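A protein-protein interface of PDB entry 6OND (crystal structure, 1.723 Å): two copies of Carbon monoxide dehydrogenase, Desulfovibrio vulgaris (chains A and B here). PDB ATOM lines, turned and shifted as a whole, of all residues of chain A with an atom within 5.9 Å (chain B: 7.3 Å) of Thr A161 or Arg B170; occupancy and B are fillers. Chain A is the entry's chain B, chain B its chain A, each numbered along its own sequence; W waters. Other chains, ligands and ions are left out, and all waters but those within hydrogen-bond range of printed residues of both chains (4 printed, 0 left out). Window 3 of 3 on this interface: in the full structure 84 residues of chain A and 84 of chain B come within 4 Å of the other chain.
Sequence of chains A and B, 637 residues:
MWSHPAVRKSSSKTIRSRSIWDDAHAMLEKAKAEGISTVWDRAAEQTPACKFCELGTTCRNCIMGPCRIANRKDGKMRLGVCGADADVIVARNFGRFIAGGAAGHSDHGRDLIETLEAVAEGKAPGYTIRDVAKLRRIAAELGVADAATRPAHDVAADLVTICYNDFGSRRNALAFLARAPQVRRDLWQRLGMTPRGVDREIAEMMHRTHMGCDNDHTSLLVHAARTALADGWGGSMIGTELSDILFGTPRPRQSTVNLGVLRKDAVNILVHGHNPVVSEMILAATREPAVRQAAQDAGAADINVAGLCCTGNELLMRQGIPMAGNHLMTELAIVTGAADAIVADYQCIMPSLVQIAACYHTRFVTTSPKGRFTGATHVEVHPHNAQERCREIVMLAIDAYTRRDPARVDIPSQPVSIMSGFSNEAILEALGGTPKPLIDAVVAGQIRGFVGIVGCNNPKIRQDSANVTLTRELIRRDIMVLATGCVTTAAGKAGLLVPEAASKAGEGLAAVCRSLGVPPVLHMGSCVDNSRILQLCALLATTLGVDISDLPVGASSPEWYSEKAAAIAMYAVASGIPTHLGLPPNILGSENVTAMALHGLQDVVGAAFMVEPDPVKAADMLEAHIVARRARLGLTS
NH2 of Arg B170 is in salt-bridge range of OE2 of Glu A117, 3.0 Å away.
NH1 of Arg B170 is in hydrogen-bond range of OG1 of Thr A161 (3.0 Å).
The side-chain carboxylate (OE1) of Glu A117 sits at hydrogen-bond distance from the side-chain hydroxyl (OH) of Tyr A164 (3.3 Å).
OG1 of Thr A161 sits at hydrogen-bond distance from O of Ala A157 (3.3 Å).
ND2 of Asn A165 lies close to O of Thr A161, at 3.4 Å.
Arg B170 touches Val A160 (NH2 to CG1, 3.8 Å).
CE1 of Tyr A164 touches O of Ser B169 (3.6 Å).
Tyr A164 touches Arg B170 (CD2 to NE, 3.3 Å).
Of chain B, only Arg B170 comes within 4 Å of Thr A161.
Arg B170 touches just these residues of chain A: Glu A117, Val A160, Thr A161 and Tyr A164.
Printed residues of chain B within 4 Å of Tyr A164: Ser B169 (3.6 Å) and Arg B170 (3.3 Å).
Printed residues of chain B within 4 Å of Val A160: Arg B170 (3.8 Å).
Of the printed residues of chain A, Ser B169 touches Tyr A164 (3.6 Å).
Phe B167 touches none of the printed residues of chain A.
Arg B200 touches none of the printed residues of chain A.
The nearest printed residue of chain B that does not touch Thr A161 is Ser B169 (9.0 Å).
The nearest residue of chain A that does not touch Arg B170 is Ala A157 (5.3 Å).
The nearest printed residue of chain B that does not touch Tyr A164 is Gly B168 (5.6 Å).
Hydrophobic or aromatic side chains of chain A that line the printed part of chain B: Val A160 and Tyr A164.
Position printed for both chains: 165.
Of the 5 pairs that touch across the chains among the printed residues, none has its exchanged pair printed and touching as well.
Water W4 bridges the side-chain carboxylate of Glu A117 (2.6 Å) and the guanidinium group of Arg B170 (3.0 Å).
Water W3 bridges O of Tyr A164 (2.8 Å) and N of Ser B169 (2.8 Å).
Water W1 lies within hydrogen-bond range of the backbone carbonyl oxygen of Ala A157 (2.8 Å), the side-chain hydroxyl of Thr A161 (3.0 Å) and the guanidinium group of Arg B170 (3.1 Å).
Water W2 bridges OD1 of Asn A165 (3.0 Å) and NH1 of Arg B170 (3.0 Å).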
ATOM      1  N   GLU A 117     -17.705 -30.059 -13.257  1.00  0.00           N
ATOM      2  CA  GLU A 117     -17.124 -28.777 -12.884  1.00  0.00           C
ATOM      3  C   GLU A 117     -16.302 -28.909 -11.617  1.00  0.00           C
ATOM      4  O   GLU A 117     -15.181 -28.401 -11.538  1.00  0.00           O
ATOM      5  CB  GLU A 117     -18.235 -27.743 -12.689  1.00  0.00           C
ATOM      6  CG  GLU A 117     -17.748 -26.358 -12.308  1.00  0.00           C
ATOM      7  CD  GLU A 117     -18.892 -25.365 -12.181  1.00  0.00           C
ATOM      8  OE1 GLU A 117     -19.942 -25.718 -11.590  1.00  0.00           O
ATOM      9  OE2 GLU A 117     -18.745 -24.230 -12.685  1.00  0.00           O
ATOM     10  N   ALA A 156     -12.149 -29.837 -19.822  1.00  0.00           N
ATOM     11  CA  ALA A 156     -13.353 -30.097 -19.033  1.00  0.00           C
ATOM     12  C   ALA A 156     -14.068 -28.805 -18.653  1.00  0.00           C
ATOM     13  O   ALA A 156     -15.301 -28.729 -18.713  1.00  0.00           O
ATOM     14  CB  ALA A 156     -12.992 -30.872 -17.758  1.00  0.00           C
ATOM     15  N   ALA A 157     -13.316 -27.783 -18.250  1.00  0.00           N
ATOM     16  CA  ALA A 157     -13.956 -26.519 -17.885  1.00  0.00           C
ATOM     17  C   ALA A 157     -14.680 -25.892 -19.073  1.00  0.00           C
ATOM     18  O   ALA A 157     -15.762 -25.314 -18.911  1.00  0.00           O
ATOM     19  CB  ALA A 157     -12.931 -25.553 -17.302  1.00  0.00           C
ATOM     20  N   ASP A 158     -14.105 -25.996 -20.273  1.00  0.00           N
ATOM     21  CA  ASP A 158     -14.755 -25.424 -21.450  1.00  0.00           C
ATOM     22  C   ASP A 158     -15.984 -26.225 -21.862  1.00  0.00           C
ATOM     23  O   ASP A 158     -16.964 -25.643 -22.353  1.00  0.00           O
ATOM     24  CB  ASP A 158     -13.771 -25.301 -22.611  1.00  0.00           C
ATOM     25  CG  ASP A 158     -12.836 -24.112 -22.460  1.00  0.00           C
ATOM     26  OD1 ASP A 158     -13.036 -23.303 -21.522  1.00  0.00           O
ATOM     27  OD2 ASP A 158     -11.905 -23.987 -23.284  1.00  0.00           O
ATOM     28  N   LEU A 159     -15.954 -27.549 -21.679  1.00  0.00           N
ATOM     29  CA  LEU A 159     -17.144 -28.350 -21.964  1.00  0.00           C
ATOM     30  C   LEU A 159     -18.258 -28.043 -20.968  1.00  0.00           C
ATOM     31  O   LEU A 159     -19.435 -27.950 -21.353  1.00  0.00           O
ATOM     32  CB  LEU A 159     -16.797 -29.843 -21.963  1.00  0.00           C
ATOM     33  CG  LEU A 159     -17.965 -30.821 -22.135  1.00  0.00           C
ATOM     34  CD1 LEU A 159     -18.709 -30.572 -23.474  1.00  0.00           C
ATOM     35  CD2 LEU A 159     -17.455 -32.264 -22.048  1.00  0.00           C
ATOM     36  N   VAL A 160     -17.903 -27.897 -19.683  1.00  0.00           N
ATOM     37  CA  VAL A 160     -18.861 -27.474 -18.662  1.00  0.00           C
ATOM     38  C   VAL A 160     -19.565 -26.189 -19.087  1.00  0.00           C
ATOM     39  O   VAL A 160     -20.785 -26.064 -18.964  1.00  0.00           O
ATOM     40  CB  VAL A 160     -18.156 -27.325 -17.299  1.00  0.00           C
ATOM     41  CG1 VAL A 160     -18.947 -26.419 -16.351  1.00  0.00           C
ATOM     42  CG2 VAL A 160     -17.933 -28.705 -16.681  1.00  0.00           C
ATOM     43  N   THR A 161     -18.810 -25.219 -19.596  1.00  0.00           N
ATOM     44  CA  THR A 161     -19.428 -23.962 -20.018  1.00  0.00           C
ATOM     45  C   THR A 161     -20.425 -24.175 -21.160  1.00  0.00           C
ATOM     46  O   THR A 161     -21.517 -23.587 -21.156  1.00  0.00           O
ATOM     47  CB  THR A 161     -18.344 -22.949 -20.390  1.00  0.00           C
ATOM     48  OG1 THR A 161     -17.601 -22.599 -19.217  1.00  0.00           O
ATOM     49  CG2 THR A 161     -18.958 -21.696 -21.011  1.00  0.00           C
ATOM     50  N   ILE A 162     -20.080 -25.033 -22.133  1.00  0.00           N
ATOM     51  CA  ILE A 162     -20.996 -25.336 -23.233  1.00  0.00           C
ATOM     52  C   ILE A 162     -22.271 -25.981 -22.711  1.00  0.00           C
ATOM     53  O   ILE A 162     -23.383 -25.609 -23.111  1.00  0.00           O
ATOM     54  CB  ILE A 162     -20.302 -26.231 -24.277  1.00  0.00           C
ATOM     55  CG1 ILE A 162     -19.283 -25.402 -25.057  1.00  0.00           C
ATOM     56  CG2 ILE A 162     -21.328 -26.854 -25.223  1.00  0.00           C
ATOM     57  CD1 ILE A 162     -18.306 -26.242 -25.837  1.00  0.00           C
ATOM     58  N   CYS A 163     -22.126 -26.976 -21.827  1.00  0.00           N
ATOM     59  CA  CYS A 163     -23.300 -27.653 -21.283  1.00  0.00           C
ATOM     60  C   CYS A 163     -24.176 -26.694 -20.481  1.00  0.00           C
ATOM     61  O   CYS A 163     -25.404 -26.693 -20.639  1.00  0.00           O
ATOM     62  CB  CYS A 163     -22.883 -28.873 -20.465  1.00  0.00           C
ATOM     63  SG  CYS A 163     -22.095 -30.178 -21.498  1.00  0.00           S
ATOM     64  N   TYR A 164     -23.565 -25.845 -19.636  1.00  0.00           N
ATOM     65  CA  TYR A 164     -24.353 -24.879 -18.875  1.00  0.00           C
ATOM     66  C   TYR A 164     -25.098 -23.901 -19.779  1.00  0.00           C
ATOM     67  O   TYR A 164     -26.227 -23.502 -19.472  1.00  0.00           O
ATOM     68  CB  TYR A 164     -23.458 -24.114 -17.901  1.00  0.00           C
ATOM     69  CG  TYR A 164     -23.352 -24.725 -16.528  1.00  0.00           C
ATOM     70  CD1 TYR A 164     -24.479 -25.162 -15.845  1.00  0.00           C
ATOM     71  CD2 TYR A 164     -22.116 -24.843 -15.904  1.00  0.00           C
ATOM     72  CE1 TYR A 164     -24.368 -25.699 -14.564  1.00  0.00           C
ATOM     73  CE2 TYR A 164     -22.003 -25.361 -14.632  1.00  0.00           C
ATOM     74  CZ  TYR A 164     -23.127 -25.796 -13.974  1.00  0.00           C
ATOM     75  OH  TYR A 164     -22.997 -26.333 -12.711  1.00  0.00           O
ATOM     76  N   ASN A 165     -24.491 -23.501 -20.898  1.00  0.00           N
ATOM     77  CA  ASN A 165     -25.187 -22.598 -21.815  1.00  0.00           C
ATOM     78  C   ASN A 165     -26.438 -23.236 -22.406  1.00  0.00           C
ATOM     79  O   ASN A 165     -27.388 -22.527 -22.760  1.00  0.00           O
ATOM     80  CB  ASN A 165     -24.241 -22.073 -22.900  1.00  0.00           C
ATOM     81  CG  ASN A 165     -23.190 -21.130 -22.329  1.00  0.00           C
ATOM     82  OD1 ASN A 165     -23.336 -20.655 -21.212  1.00  0.00           O
ATOM     83  ND2 ASN A 165     -22.126 -20.872 -23.081  1.00  0.00           N
ATOM     84  N   ASP A 166     -26.471 -24.566 -22.515  1.00  0.00           N
ATOM     85  CA  ASP A 166     -27.700 -25.238 -22.916  1.00  0.00           C
ATOM     86  C   ASP A 166     -28.773 -25.199 -21.837  1.00  0.00           C
ATOM     87  O   ASP A 166     -29.953 -25.409 -22.148  1.00  0.00           O
ATOM     88  CB  ASP A 166     -27.410 -26.673 -23.366  1.00  0.00           C
ATOM     89  CG  ASP A 166     -27.058 -26.756 -24.853  1.00  0.00           C
ATOM     90  OD1 ASP A 166     -26.911 -25.686 -25.493  1.00  0.00           O
ATOM     91  OD2 ASP A 166     -26.951 -27.883 -25.386  1.00  0.00           O
ATOM     92  N   ASN B 165     -27.970 -14.249 -17.490  1.00  0.00           N
ATOM     93  CA  ASN B 165     -27.308 -15.145 -16.547  1.00  0.00           C
ATOM     94  C   ASN B 165     -28.228 -15.528 -15.393  1.00  0.00           C
ATOM     95  O   ASN B 165     -28.097 -16.622 -14.838  1.00  0.00           O
ATOM     96  CB  ASN B 165     -26.006 -14.524 -16.044  1.00  0.00           C
ATOM     97  CG  ASN B 165     -24.932 -14.481 -17.123  1.00  0.00           C
ATOM     98  OD1 ASN B 165     -25.048 -15.139 -18.157  1.00  0.00           O
ATOM     99  ND2 ASN B 165     -23.887 -13.696 -16.887  1.00  0.00           N
ATOM    100  N   PHE B 167     -31.295 -16.223 -15.871  1.00  0.00           N
ATOM    101  CA  PHE B 167     -32.033 -17.314 -16.497  1.00  0.00           C
ATOM    102  C   PHE B 167     -31.126 -18.477 -16.884  1.00  0.00           C
ATOM    103  O   PHE B 167     -31.486 -19.290 -17.743  1.00  0.00           O
ATOM    104  CB  PHE B 167     -32.791 -16.801 -17.726  1.00  0.00           C
ATOM    105  CG  PHE B 167     -34.033 -16.008 -17.400  1.00  0.00           C
ATOM    106  CD1 PHE B 167     -33.946 -14.679 -17.013  1.00  0.00           C
ATOM    107  CD2 PHE B 167     -35.286 -16.602 -17.471  1.00  0.00           C
ATOM    108  CE1 PHE B 167     -35.081 -13.953 -16.712  1.00  0.00           C
ATOM    109  CE2 PHE B 167     -36.442 -15.876 -17.189  1.00  0.00           C
ATOM    110  CZ  PHE B 167     -36.337 -14.549 -16.804  1.00  0.00           C
ATOM    111  N   GLY B 168     -29.939 -18.552 -16.296  1.00  0.00           N
ATOM    112  CA  GLY B 168     -29.053 -19.672 -16.467  1.00  0.00           C
ATOM    113  C   GLY B 168     -28.890 -20.443 -15.171  1.00  0.00           C
ATOM    114  O   GLY B 168     -29.615 -20.249 -14.192  1.00  0.00           O
ATOM    115  N   SER B 169     -27.887 -21.303 -15.161  1.00  0.00           N
ATOM    116  CA  SER B 169     -27.772 -22.291 -14.097  1.00  0.00           C
ATOM    117  C   SER B 169     -26.453 -22.192 -13.336  1.00  0.00           C
ATOM    118  O   SER B 169     -26.068 -23.146 -12.656  1.00  0.00           O
ATOM    119  CB  SER B 169     -27.995 -23.699 -14.673  1.00  0.00           C
ATOM    120  OG  SER B 169     -28.116 -24.655 -13.637  1.00  0.00           O
ATOM    121  N   ARG B 170     -25.765 -21.049 -13.392  1.00  0.00           N
ATOM    122  CA  ARG B 170     -24.446 -20.937 -12.780  1.00  0.00           C
ATOM    123  C   ARG B 170     -24.382 -20.005 -11.577  1.00  0.00           C
ATOM    124  O   ARG B 170     -23.320 -19.900 -10.958  1.00  0.00           O
ATOM    125  CB  ARG B 170     -23.399 -20.509 -13.817  1.00  0.00           C
ATOM    126  CG  ARG B 170     -23.315 -21.471 -15.023  1.00  0.00           C
ATOM    127  CD  ARG B 170     -22.046 -21.225 -15.835  1.00  0.00           C
ATOM    128  NE  ARG B 170     -20.884 -21.889 -15.240  1.00  0.00           N
ATOM    129  CZ  ARG B 170     -19.763 -22.175 -15.902  1.00  0.00           C
ATOM    130  NH1 ARG B 170     -19.640 -21.860 -17.189  1.00  0.00           N
ATOM    131  NH2 ARG B 170     -18.766 -22.805 -15.279  1.00  0.00           N
ATOM    132  N   ARG B 171     -25.468 -19.339 -11.216  1.00  0.00           N
ATOM    133  CA  ARG B 171     -25.389 -18.385 -10.120  1.00  0.00           C
ATOM    134  C   ARG B 171     -25.708 -19.040  -8.784  1.00  0.00           C
ATOM    135  O   ARG B 171     -26.440 -20.031  -8.705  1.00  0.00           O
ATOM    136  CB  ARG B 171     -26.331 -17.211 -10.363  1.00  0.00           C
ATOM    137  CG  ARG B 171     -25.878 -16.347 -11.505  1.00  0.00           C
ATOM    138  CD  ARG B 171     -26.639 -15.055 -11.553  1.00  0.00           C
ATOM    139  NE  ARG B 171     -26.499 -14.249 -10.335  1.00  0.00           N
ATOM    140  CZ  ARG B 171     -25.459 -13.469 -10.070  1.00  0.00           C
ATOM    141  NH1 ARG B 171     -25.415 -12.773  -8.936  1.00  0.00           N
ATOM    142  NH2 ARG B 171     -24.457 -13.389 -10.934  1.00  0.00           N
ATOM    143  N   ASN B 172     -25.137 -18.476  -7.721  1.00  0.00           N
ATOM    144  CA  ASN B 172     -25.529 -18.883  -6.386  1.00  0.00           C
ATOM    145  C   ASN B 172     -26.710 -18.082  -5.861  1.00  0.00           C
ATOM    146  O   ASN B 172     -27.395 -18.547  -4.941  1.00  0.00           O
ATOM    147  CB  ASN B 172     -24.347 -18.781  -5.425  1.00  0.00           C
ATOM    148  CG  ASN B 172     -23.231 -19.725  -5.796  1.00  0.00           C
ATOM    149  OD1 ASN B 172     -23.480 -20.870  -6.172  1.00  0.00           O
ATOM    150  ND2 ASN B 172     -21.994 -19.248  -5.713  1.00  0.00           N
ATOM    151  N   ALA B 173     -26.983 -16.915  -6.444  1.00  0.00           N
ATOM    152  CA  ALA B 173     -28.098 -16.067  -6.040  1.00  0.00           C
ATOM    153  C   ALA B 173     -28.400 -15.087  -7.169  1.00  0.00           C
ATOM    154  O   ALA B 173     -27.482 -14.578  -7.823  1.00  0.00           O
ATOM    155  CB  ALA B 173     -27.746 -15.265  -4.787  1.00  0.00           C
ATOM    156  N   ARG B 196     -31.717 -19.087  -7.175  1.00  0.00           N
ATOM    157  CA  ARG B 196     -30.449 -19.171  -7.909  1.00  0.00           C
ATOM    158  C   ARG B 196     -30.589 -18.916  -9.401  1.00  0.00           C
ATOM    159  O   ARG B 196     -29.693 -18.326 -10.019  1.00  0.00           O
ATOM    160  CB  ARG B 196     -29.827 -20.558  -7.737  1.00  0.00           C
ATOM    161  CG  ARG B 196     -29.656 -21.007  -6.292  1.00  0.00           C
ATOM    162  CD  ARG B 196     -29.555 -22.527  -6.228  1.00  0.00           C
ATOM    163  NE  ARG B 196     -30.834 -23.185  -6.507  1.00  0.00           N
ATOM    164  CZ  ARG B 196     -31.012 -24.507  -6.485  1.00  0.00           C
ATOM    165  NH1 ARG B 196     -29.994 -25.314  -6.199  1.00  0.00           N
ATOM    166  NH2 ARG B 196     -32.207 -25.021  -6.738  1.00  0.00           N
ATOM    167  N   GLY B 197     -31.677 -19.373  -9.997  1.00  0.00           N
ATOM    168  CA  GLY B 197     -31.910 -19.202 -11.421  1.00  0.00           C
ATOM    169  C   GLY B 197     -33.398 -19.152 -11.640  1.00  0.00           C
ATOM    170  O   GLY B 197     -34.121 -19.955 -11.051  1.00  0.00           O
ATOM    171  N   ARG B 200     -34.378 -22.235 -13.469  1.00  0.00           N
ATOM    172  CA  ARG B 200     -33.899 -23.410 -12.738  1.00  0.00           C
ATOM    173  C   ARG B 200     -34.863 -23.823 -11.629  1.00  0.00           C
ATOM    174  O   ARG B 200     -35.141 -25.018 -11.450  1.00  0.00           O
ATOM    175  CB  ARG B 200     -32.500 -23.164 -12.175  1.00  0.00           C
ATOM    176  CG  ARG B 200     -32.047 -24.306 -11.259  1.00  0.00           C
ATOM    177  CD  ARG B 200     -30.625 -24.150 -10.761  1.00  0.00           C
ATOM    178  NE  ARG B 200     -30.231 -25.380 -10.084  1.00  0.00           N
ATOM    179  CZ  ARG B 200     -29.046 -25.597  -9.522  1.00  0.00           C
ATOM    180  NH1 ARG B 200     -28.105 -24.655  -9.532  1.00  0.00           N
ATOM    181  NH2 ARG B 200     -28.807 -26.773  -8.952  1.00  0.00           N
HETATM  182  O   HOH W   1     -16.208 -23.631 -16.740  1.00  0.00           O
HETATM  183  O   HOH W   2     -21.434 -20.288 -18.972  1.00  0.00           O
HETATM  184  O   HOH W   3     -26.241 -21.606 -17.437  1.00  0.00           O
HETATM  185  O   HOH W   4     -20.606 -22.490 -12.344  1.00  0.00           O
